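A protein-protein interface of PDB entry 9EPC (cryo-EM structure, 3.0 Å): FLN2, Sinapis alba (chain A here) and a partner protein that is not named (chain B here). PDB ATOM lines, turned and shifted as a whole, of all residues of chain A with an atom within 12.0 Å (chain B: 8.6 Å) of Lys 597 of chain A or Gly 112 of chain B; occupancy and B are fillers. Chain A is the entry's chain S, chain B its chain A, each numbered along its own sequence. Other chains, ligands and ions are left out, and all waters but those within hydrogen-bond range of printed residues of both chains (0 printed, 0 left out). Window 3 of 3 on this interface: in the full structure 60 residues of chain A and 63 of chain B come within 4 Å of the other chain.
Lys 597 of chain A touches just these residues of chain B: Gln 111, Gly 112 and Pro 113.
Of chain A, only Lys 597 (3.3 Å) comes within 4 Å of Gly 112 of chain B.
Leu 598 of chain A touches just these residues of chain B: Val 110 (3.6 Å), Gln 111 (3.1 Å), Pro 113 (3.7 Å), Gly 114 (3.4 Å), Tyr 115 (3.5 Å) and Ile 116 (3.7 Å).
Gln 111 of chain B touches just these residues of chain A: Tyr 595 (3.9 Å), Arg 596 (2.5 Å), Lys 597 (3.6 Å) and Leu 598 (3.1 Å).
Of chain A, only Lys 597 (3.5 Å), Leu 598 (3.7 Å) and Glu 599 (3.8 Å) come within 4 Å of Pro 113 of chain B.
Gly 114 of chain B touches just these residues of chain A: Leu 598 and Glu 599.
No residue of chain A comes within 4 Å of Pro 142 of chain B.
No residue of chain A comes within 4 Å of Ile 143 of chain B.
Asn 144 of chain B touches just one residue of chain A: Tyr 595 (3.2 Å).
Of the printed residues of chain A, Tyr 115 of chain B touches Leu 598.
Of the printed residues of chain A, Ile 116 of chain B touches Leu 598 (3.7 Å).
Of the printed residues of chain B, Glu 599 of chain A touches Pro 113 (3.8 Å) and Gly 114 (3.9 Å).
Of the printed residues of chain B, Arg 596 of chain A touches Cys 109 (3.7 Å), Val 110 (3.3 Å), Gln 111 (2.5 Å) and Asp 120 (3.9 Å).
Printed residues of chain A within 4 Å of Cys 109 of chain B: Arg 593 (3.1 Å), Tyr 595 (3.4 Å) and Arg 596 (3.7 Å).
Gly 79 of chain B touches none of the printed residues of chain A.
Leu 145 of chain B touches none of the printed residues of chain A.
The nearest residue of chain A that does not touch Gly 112 of chain B is Leu 598 of chain A (4.2 Å).
The nearest printed residue of chain B that does not touch Arg 596 of chain A is Arg 119 of chain B (4.1 Å).
Of the 7 printed residues of chain A, 6 touch a printed residue of chain B.
Hydrophobic or aromatic side chains of chain A within 4 Å of the printed part of chain B: Tyr 595 and Leu 598.
Of the 19 printed residues of chain B, 10 touch a printed residue of chain A.
Among the printed residues, 20 pairs touch across the chains.
Among the printed residues, Asp or Glu carboxylates within 4 Å of a Lys or Arg side-chain nitrogen of the other chain: Arg 596 of chain A with Asp 120 of chain B.
CD1 of Tyr 595 of chain A touches SG of Cys 109 of chain B, 3.4 Å away.
CB of Gln 111 of chain B touches CB of Tyr 595 of chain A (3.9 Å).
Asn 144 of chain B touches Tyr 595 of chain A.
Cys 109 of chain B touches Arg 596 of chain A.
CD of Lys 597 of chain A touches OE1 of Gln 111 of chain B, 3.6 Å away.
NZ of Lys 597 of chain A touches O of Pro 113 of chain B (3.5 Å).
Leu 598 of chain A touches Val 110 of chain B (CD1 to CB, 3.6 Å).
Pro 113 of chain B touches Leu 598 of chain A (O to CB, 3.7 Å).
Pro 113 of chain B touches Glu 599 of chain A (O to O, 3.8 Å).
Glu 599 of chain A touches Gly 114 of chain B (OE2 to CA, 3.9 Å).
N of Leu 598 of chain A is in hydrogen-bond range of O of Gln 111 of chain B (3.1 Å).
O of Arg 593 of chain A is in hydrogen-bond range of SG of Cys 109 of chain B (3.1 Å).
The guanidinium group (NH1) of Arg 596 of chain A is in salt-bridge range of the side-chain carboxylate (OD1) of Asp 120 of chain B (3.9 Å).
The backbone carbonyl oxygen of Arg 596 of chain A lies within hydrogen-bond range of the backbone NH of Gln 111 of chain B.
The backbone NH of Gly 112 of chain B sits at hydrogen-bond distance from the backbone carbonyl oxygen of Ile 143 of chain B.
The backbone carbonyl oxygen (O) of Gly 114 of chain B lies within hydrogen-bond range of the backbone NH (N) of Leu 139 of chain B (2.6 Å).
The side-chain hydroxyl (OH) of Tyr 595 of chain A sits at hydrogen-bond distance from the guanidinium group (NH1) of Arg 593 of chain A (3.0 Å).
The side-chain amide nitrogen (NE2) of Gln 111 of chain B sits at hydrogen-bond distance from the side-chain amide oxygen (OD1) of Asn 144 of chain B (2.6 Å).
The backbone carbonyl oxygen of Leu 145 of chain B sits at hydrogen-bond distance from the backbone NH of Val 110 of chain B.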
ATOM      1  N   ARG A 593       0.570  -9.381 -29.002  1.00  0.00           N
ATOM      2  CA  ARG A 593       1.142  -9.658 -27.688  1.00  0.00           C
ATOM      3  C   ARG A 593       1.276  -8.400 -26.840  1.00  0.00           C
ATOM      4  O   ARG A 593       1.168  -8.479 -25.611  1.00  0.00           O
ATOM      5  CB  ARG A 593       2.503 -10.329 -27.837  1.00  0.00           C
ATOM      6  CG  ARG A 593       2.426 -11.805 -28.142  1.00  0.00           C
ATOM      7  CD  ARG A 593       2.004 -12.601 -26.925  1.00  0.00           C
ATOM      8  NE  ARG A 593       1.765 -13.999 -27.259  1.00  0.00           N
ATOM      9  CZ  ARG A 593       2.722 -14.893 -27.463  1.00  0.00           C
ATOM     10  NH1 ARG A 593       4.001 -14.567 -27.381  1.00  0.00           N
ATOM     11  NH2 ARG A 593       2.386 -16.145 -27.760  1.00  0.00           N
ATOM     12  N   GLU A 594       1.506  -7.250 -27.471  1.00  0.00           N
ATOM     13  CA  GLU A 594       1.738  -5.964 -26.804  1.00  0.00           C
ATOM     14  C   GLU A 594       2.639  -6.127 -25.576  1.00  0.00           C
ATOM     15  O   GLU A 594       2.257  -5.858 -24.437  1.00  0.00           O
ATOM     16  CB  GLU A 594       0.419  -5.260 -26.453  1.00  0.00           C
ATOM     17  CG  GLU A 594      -0.570  -6.023 -25.575  1.00  0.00           C
ATOM     18  CD  GLU A 594      -1.807  -5.212 -25.250  1.00  0.00           C
ATOM     19  OE1 GLU A 594      -1.974  -4.120 -25.832  1.00  0.00           O
ATOM     20  OE2 GLU A 594      -2.612  -5.666 -24.410  1.00  0.00           O
ATOM     21  N   TYR A 595       3.862  -6.586 -25.842  1.00  0.00           N
ATOM     22  CA  TYR A 595       4.842  -6.798 -24.784  1.00  0.00           C
ATOM     23  C   TYR A 595       5.103  -5.501 -24.029  1.00  0.00           C
ATOM     24  O   TYR A 595       5.565  -4.516 -24.612  1.00  0.00           O
ATOM     25  CB  TYR A 595       6.148  -7.329 -25.373  1.00  0.00           C
ATOM     26  CG  TYR A 595       6.026  -8.647 -26.102  1.00  0.00           C
ATOM     27  CD1 TYR A 595       5.949  -9.843 -25.404  1.00  0.00           C
ATOM     28  CD2 TYR A 595       6.014  -8.697 -27.488  1.00  0.00           C
ATOM     29  CE1 TYR A 595       5.845 -11.051 -26.065  1.00  0.00           C
ATOM     30  CE2 TYR A 595       5.915  -9.900 -28.158  1.00  0.00           C
ATOM     31  CZ  TYR A 595       5.830 -11.074 -27.441  1.00  0.00           C
ATOM     32  OH  TYR A 595       5.727 -12.275 -28.102  1.00  0.00           O
ATOM     33  N   ARG A 596       4.809  -5.502 -22.732  1.00  0.00           N
ATOM     34  CA  ARG A 596       5.101  -4.339 -21.908  1.00  0.00           C
ATOM     35  C   ARG A 596       6.605  -4.185 -21.725  1.00  0.00           C
ATOM     36  O   ARG A 596       7.340  -5.171 -21.629  1.00  0.00           O
ATOM     37  CB  ARG A 596       4.422  -4.457 -20.545  1.00  0.00           C
ATOM     38  CG  ARG A 596       4.515  -3.190 -19.711  1.00  0.00           C
ATOM     39  CD  ARG A 596       4.572  -3.490 -18.225  1.00  0.00           C
ATOM     40  NE  ARG A 596       3.386  -4.198 -17.758  1.00  0.00           N
ATOM     41  CZ  ARG A 596       3.130  -4.467 -16.485  1.00  0.00           C
ATOM     42  NH1 ARG A 596       3.955  -4.092 -15.521  1.00  0.00           N
ATOM     43  NH2 ARG A 596       2.018  -5.123 -16.173  1.00  0.00           N
ATOM     44  N   LYS A 597       7.061  -2.938 -21.681  1.00  0.00           N
ATOM     45  CA  LYS A 597       8.467  -2.656 -21.439  1.00  0.00           C
ATOM     46  C   LYS A 597       8.748  -2.631 -19.942  1.00  0.00           C
ATOM     47  O   LYS A 597       7.925  -2.167 -19.148  1.00  0.00           O
ATOM     48  CB  LYS A 597       8.858  -1.321 -22.074  1.00  0.00           C
ATOM     49  CG  LYS A 597      10.333  -0.983 -21.961  1.00  0.00           C
ATOM     50  CD  LYS A 597      11.191  -2.030 -22.645  1.00  0.00           C
ATOM     51  CE  LYS A 597      12.668  -1.717 -22.484  1.00  0.00           C
ATOM     52  NZ  LYS A 597      13.074  -1.693 -21.052  1.00  0.00           N
ATOM     53  N   LEU A 598       9.916  -3.140 -19.561  1.00  0.00           N
ATOM     54  CA  LEU A 598      10.334  -3.148 -18.165  1.00  0.00           C
ATOM     55  C   LEU A 598      10.845  -1.761 -17.779  1.00  0.00           C
ATOM     56  O   LEU A 598      10.718  -0.792 -18.533  1.00  0.00           O
ATOM     57  CB  LEU A 598      11.383  -4.231 -17.935  1.00  0.00           C
ATOM     58  CG  LEU A 598      10.908  -5.490 -17.211  1.00  0.00           C
ATOM     59  CD1 LEU A 598       9.613  -5.996 -17.812  1.00  0.00           C
ATOM     60  CD2 LEU A 598      11.972  -6.568 -17.264  1.00  0.00           C
ATOM     61  N   GLU A 599      11.428  -1.652 -16.590  1.00  0.00           N
ATOM     62  CA  GLU A 599      11.963  -0.384 -16.108  1.00  0.00           C
ATOM     63  C   GLU A 599      13.107   0.104 -16.991  1.00  0.00           C
ATOM     64  O   GLU A 599      13.769  -0.689 -17.661  1.00  0.00           O
ATOM     65  CB  GLU A 599      12.433  -0.519 -14.656  1.00  0.00           C
ATOM     66  CG  GLU A 599      13.493  -1.591 -14.428  1.00  0.00           C
ATOM     67  CD  GLU A 599      14.907  -1.082 -14.644  1.00  0.00           C
ATOM     68  OE1 GLU A 599      15.100   0.152 -14.675  1.00  0.00           O
ATOM     69  OE2 GLU A 599      15.827  -1.916 -14.783  1.00  0.00           O
ATOM     70  N   GLY B  79      19.380 -14.113 -22.873  1.00  0.00           N
ATOM     71  CA  GLY B  79      18.929 -12.845 -22.346  1.00  0.00           C
ATOM     72  C   GLY B  79      18.413 -12.896 -20.926  1.00  0.00           C
ATOM     73  O   GLY B  79      18.188 -11.837 -20.330  1.00  0.00           O
ATOM     74  N   CYS B 109       3.383 -11.305 -19.782  1.00  0.00           N
ATOM     75  CA  CYS B 109       3.826 -10.854 -21.099  1.00  0.00           C
ATOM     76  C   CYS B 109       4.502  -9.495 -20.968  1.00  0.00           C
ATOM     77  O   CYS B 109       3.838  -8.467 -20.825  1.00  0.00           O
ATOM     78  CB  CYS B 109       2.641 -10.786 -22.053  1.00  0.00           C
ATOM     79  SG  CYS B 109       3.028 -10.128 -23.680  1.00  0.00           S
ATOM     80  N   VAL B 110       5.834  -9.485 -21.023  1.00  0.00           N
ATOM     81  CA  VAL B 110       6.640  -8.278 -20.914  1.00  0.00           C
ATOM     82  C   VAL B 110       7.832  -8.403 -21.855  1.00  0.00           C
ATOM     83  O   VAL B 110       8.029  -9.427 -22.512  1.00  0.00           O
ATOM     84  CB  VAL B 110       7.127  -8.020 -19.472  1.00  0.00           C
ATOM     85  CG1 VAL B 110       5.961  -7.743 -18.537  1.00  0.00           C
ATOM     86  CG2 VAL B 110       7.954  -9.194 -18.977  1.00  0.00           C
ATOM     87  N   GLN B 111       8.633  -7.341 -21.921  1.00  0.00           N
ATOM     88  CA  GLN B 111       9.896  -7.365 -22.642  1.00  0.00           C
ATOM     89  C   GLN B 111      10.938  -6.603 -21.839  1.00  0.00           C
ATOM     90  O   GLN B 111      10.609  -5.706 -21.058  1.00  0.00           O
ATOM     91  CB  GLN B 111       9.774  -6.766 -24.048  1.00  0.00           C
ATOM     92  CG  GLN B 111       9.671  -5.255 -24.079  1.00  0.00           C
ATOM     93  CD  GLN B 111       9.840  -4.694 -25.474  1.00  0.00           C
ATOM     94  OE1 GLN B 111       9.862  -3.480 -25.668  1.00  0.00           O
ATOM     95  NE2 GLN B 111       9.964  -5.579 -26.456  1.00  0.00           N
ATOM     96  N   GLY B 112      12.202  -6.970 -22.035  1.00  0.00           N
ATOM     97  CA  GLY B 112      13.283  -6.397 -21.271  1.00  0.00           C
ATOM     98  C   GLY B 112      14.087  -5.376 -22.048  1.00  0.00           C
ATOM     99  O   GLY B 112      13.629  -4.827 -23.054  1.00  0.00           O
ATOM    100  N   PRO B 113      15.317  -5.105 -21.595  1.00  0.00           N
ATOM    101  CA  PRO B 113      15.997  -5.674 -20.419  1.00  0.00           C
ATOM    102  C   PRO B 113      15.483  -5.102 -19.103  1.00  0.00           C
ATOM    103  O   PRO B 113      14.852  -4.050 -19.082  1.00  0.00           O
ATOM    104  CB  PRO B 113      17.473  -5.297 -20.649  1.00  0.00           C
ATOM    105  CG  PRO B 113      17.569  -4.862 -22.089  1.00  0.00           C
ATOM    106  CD  PRO B 113      16.230  -4.270 -22.387  1.00  0.00           C
ATOM    107  N   GLY B 114      15.739  -5.776 -17.994  1.00  0.00           N
ATOM    108  CA  GLY B 114      15.328  -5.291 -16.696  1.00  0.00           C
ATOM    109  C   GLY B 114      15.070  -6.450 -15.753  1.00  0.00           C
ATOM    110  O   GLY B 114      15.443  -7.588 -16.019  1.00  0.00           O
ATOM    111  N   TYR B 115      14.415  -6.126 -14.643  1.00  0.00           N
ATOM    112  CA  TYR B 115      14.045  -7.105 -13.631  1.00  0.00           C
ATOM    113  C   TYR B 115      12.557  -7.404 -13.736  1.00  0.00           C
ATOM    114  O   TYR B 115      11.734  -6.484 -13.752  1.00  0.00           O
ATOM    115  CB  TYR B 115      14.370  -6.591 -12.229  1.00  0.00           C
ATOM    116  CG  TYR B 115      15.840  -6.585 -11.894  1.00  0.00           C
ATOM    117  CD1 TYR B 115      16.434  -5.475 -11.313  1.00  0.00           C
ATOM    118  CD2 TYR B 115      16.632  -7.696 -12.142  1.00  0.00           C
ATOM    119  CE1 TYR B 115      17.776  -5.465 -10.998  1.00  0.00           C
ATOM    120  CE2 TYR B 115      17.976  -7.696 -11.830  1.00  0.00           C
ATOM    121  CZ  TYR B 115      18.543  -6.579 -11.260  1.00  0.00           C
ATOM    122  OH  TYR B 115      19.883  -6.574 -10.948  1.00  0.00           O
ATOM    123  N   ILE B 116      12.216  -8.686 -13.804  1.00  0.00           N
ATOM    124  CA  ILE B 116      10.823  -9.115 -13.789  1.00  0.00           C
ATOM    125  C   ILE B 116      10.445  -9.428 -12.350  1.00  0.00           C
ATOM    126  O   ILE B 116      11.054 -10.293 -11.713  1.00  0.00           O
ATOM    127  CB  ILE B 116      10.600 -10.333 -14.694  1.00  0.00           C
ATOM    128  CG1 ILE B 116      10.923  -9.989 -16.146  1.00  0.00           C
ATOM    129  CG2 ILE B 116       9.168 -10.814 -14.579  1.00  0.00           C
ATOM    130  CD1 ILE B 116      10.611 -11.108 -17.110  1.00  0.00           C
ATOM    131  N   ARG B 119       5.096  -7.641  -9.509  1.00  0.00           N
ATOM    132  CA  ARG B 119       4.268  -6.527  -9.956  1.00  0.00           C
ATOM    133  C   ARG B 119       3.990  -6.568 -11.452  1.00  0.00           C
ATOM    134  O   ARG B 119       3.064  -5.894 -11.913  1.00  0.00           O
ATOM    135  CB  ARG B 119       4.945  -5.208  -9.583  1.00  0.00           C
ATOM    136  CG  ARG B 119       4.055  -3.981  -9.679  1.00  0.00           C
ATOM    137  CD  ARG B 119       4.824  -2.708  -9.357  1.00  0.00           C
ATOM    138  NE  ARG B 119       5.905  -2.460 -10.304  1.00  0.00           N
ATOM    139  CZ  ARG B 119       7.181  -2.742 -10.077  1.00  0.00           C
ATOM    140  NH1 ARG B 119       7.577  -3.280  -8.937  1.00  0.00           N
ATOM    141  NH2 ARG B 119       8.081  -2.476 -11.019  1.00  0.00           N
ATOM    142  N   ASP B 120       4.754  -7.347 -12.213  1.00  0.00           N
ATOM    143  CA  ASP B 120       4.612  -7.422 -13.658  1.00  0.00           C
ATOM    144  C   ASP B 120       3.646  -8.511 -14.103  1.00  0.00           C
ATOM    145  O   ASP B 120       3.508  -8.745 -15.307  1.00  0.00           O
ATOM    146  CB  ASP B 120       5.980  -7.649 -14.301  1.00  0.00           C
ATOM    147  CG  ASP B 120       7.052  -6.762 -13.705  1.00  0.00           C
ATOM    148  OD1 ASP B 120       6.724  -5.634 -13.282  1.00  0.00           O
ATOM    149  OD2 ASP B 120       8.221  -7.194 -13.651  1.00  0.00           O
ATOM    150  N   THR B 138      15.475 -11.993 -14.425  1.00  0.00           N
ATOM    151  CA  THR B 138      16.307 -10.866 -14.821  1.00  0.00           C
ATOM    152  C   THR B 138      16.535 -10.941 -16.322  1.00  0.00           C
ATOM    153  O   THR B 138      17.026 -11.956 -16.825  1.00  0.00           O
ATOM    154  CB  THR B 138      17.643 -10.874 -14.079  1.00  0.00           C
ATOM    155  OG1 THR B 138      17.414 -10.689 -12.677  1.00  0.00           O
ATOM    156  CG2 THR B 138      18.540  -9.764 -14.595  1.00  0.00           C
ATOM    157  N   LEU B 139      16.181  -9.875 -17.030  1.00  0.00           N
ATOM    158  CA  LEU B 139      16.369  -9.799 -18.470  1.00  0.00           C
ATOM    159  C   LEU B 139      17.563  -8.906 -18.773  1.00  0.00           C
ATOM    160  O   LEU B 139      17.613  -7.755 -18.329  1.00  0.00           O
ATOM    161  CB  LEU B 139      15.115  -9.263 -19.160  1.00  0.00           C
ATOM    162  CG  LEU B 139      13.848 -10.087 -18.933  1.00  0.00           C
ATOM    163  CD1 LEU B 139      12.722  -9.614 -19.830  1.00  0.00           C
ATOM    164  CD2 LEU B 139      14.130 -11.551 -19.168  1.00  0.00           C
ATOM    165  N   THR B 140      18.522  -9.442 -19.526  1.00  0.00           N
ATOM    166  CA  THR B 140      19.745  -8.717 -19.843  1.00  0.00           C
ATOM    167  C   THR B 140      19.727  -8.079 -21.222  1.00  0.00           C
ATOM    168  O   THR B 140      20.435  -7.091 -21.441  1.00  0.00           O
ATOM    169  CB  THR B 140      20.955  -9.649 -19.739  1.00  0.00           C
ATOM    170  OG1 THR B 140      20.791 -10.748 -20.645  1.00  0.00           O
ATOM    171  CG2 THR B 140      21.092 -10.184 -18.323  1.00  0.00           C
ATOM    172  N   GLU B 141      18.946  -8.609 -22.151  1.00  0.00           N
ATOM    173  CA  GLU B 141      18.839  -8.075 -23.498  1.00  0.00           C
ATOM    174  C   GLU B 141      17.372  -7.925 -23.859  1.00  0.00           C
ATOM    175  O   GLU B 141      16.512  -8.620 -23.306  1.00  0.00           O
ATOM    176  CB  GLU B 141      19.550  -8.983 -24.513  1.00  0.00           C
ATOM    177  CG  GLU B 141      18.838 -10.285 -24.807  1.00  0.00           C
ATOM    178  CD  GLU B 141      19.580 -11.135 -25.820  1.00  0.00           C
ATOM    179  OE1 GLU B 141      20.796 -10.918 -26.002  1.00  0.00           O
ATOM    180  OE2 GLU B 141      18.947 -12.016 -26.437  1.00  0.00           O
ATOM    181  N   PRO B 142      17.046  -7.015 -24.784  1.00  0.00           N
ATOM    182  CA  PRO B 142      15.632  -6.746 -25.082  1.00  0.00           C
ATOM    183  C   PRO B 142      14.939  -7.889 -25.803  1.00  0.00           C
ATOM    184  O   PRO B 142      14.709  -7.824 -27.015  1.00  0.00           O
ATOM    185  CB  PRO B 142      15.694  -5.491 -25.959  1.00  0.00           C
ATOM    186  CG  PRO B 142      17.041  -5.545 -26.586  1.00  0.00           C
ATOM    187  CD  PRO B 142      17.943  -6.126 -25.541  1.00  0.00           C
ATOM    188  N   ILE B 143      14.601  -8.940 -25.064  1.00  0.00           N
ATOM    189  CA  ILE B 143      13.813 -10.038 -25.589  1.00  0.00           C
ATOM    190  C   ILE B 143      12.376  -9.867 -25.123  1.00  0.00           C
ATOM    191  O   ILE B 143      12.083  -9.152 -24.162  1.00  0.00           O
ATOM    192  CB  ILE B 143      14.369 -11.411 -25.155  1.00  0.00           C
ATOM    193  CG1 ILE B 143      14.522 -11.458 -23.635  1.00  0.00           C
ATOM    194  CG2 ILE B 143      15.687 -11.696 -25.848  1.00  0.00           C
ATOM    195  CD1 ILE B 143      14.915 -12.814 -23.103  1.00  0.00           C
ATOM    196  N   ASN B 144      11.461 -10.541 -25.813  1.00  0.00           N
ATOM    197  CA  ASN B 144      10.042 -10.507 -25.480  1.00  0.00           C
ATOM    198  C   ASN B 144       9.678 -11.823 -24.806  1.00  0.00           C
ATOM    199  O   ASN B 144       9.661 -12.875 -25.452  1.00  0.00           O
ATOM    200  CB  ASN B 144       9.200 -10.275 -26.730  1.00  0.00           C
ATOM    201  CG  ASN B 144       9.550  -8.982 -27.435  1.00  0.00           C
ATOM    202  OD1 ASN B 144       9.060  -7.912 -27.076  1.00  0.00           O
ATOM    203  ND2 ASN B 144      10.404  -9.074 -28.447  1.00  0.00           N
ATOM    204  N   LEU B 145       9.385 -11.763 -23.511  1.00  0.00           N
ATOM    205  CA  LEU B 145       9.068 -12.944 -22.719  1.00  0.00           C
ATOM    206  C   LEU B 145       7.604 -12.910 -22.313  1.00  0.00           C
ATOM    207  O   LEU B 145       7.142 -11.934 -21.712  1.00  0.00           O
ATOM    208  CB  LEU B 145       9.955 -13.024 -21.477  1.00  0.00           C
ATOM    209  CG  LEU B 145       9.625 -14.168 -20.519  1.00  0.00           C
ATOM    210  CD1 LEU B 145       9.763 -15.506 -21.224  1.00  0.00           C
ATOM    211  CD2 LEU B 145      10.512 -14.115 -19.289  1.00  0.00           C
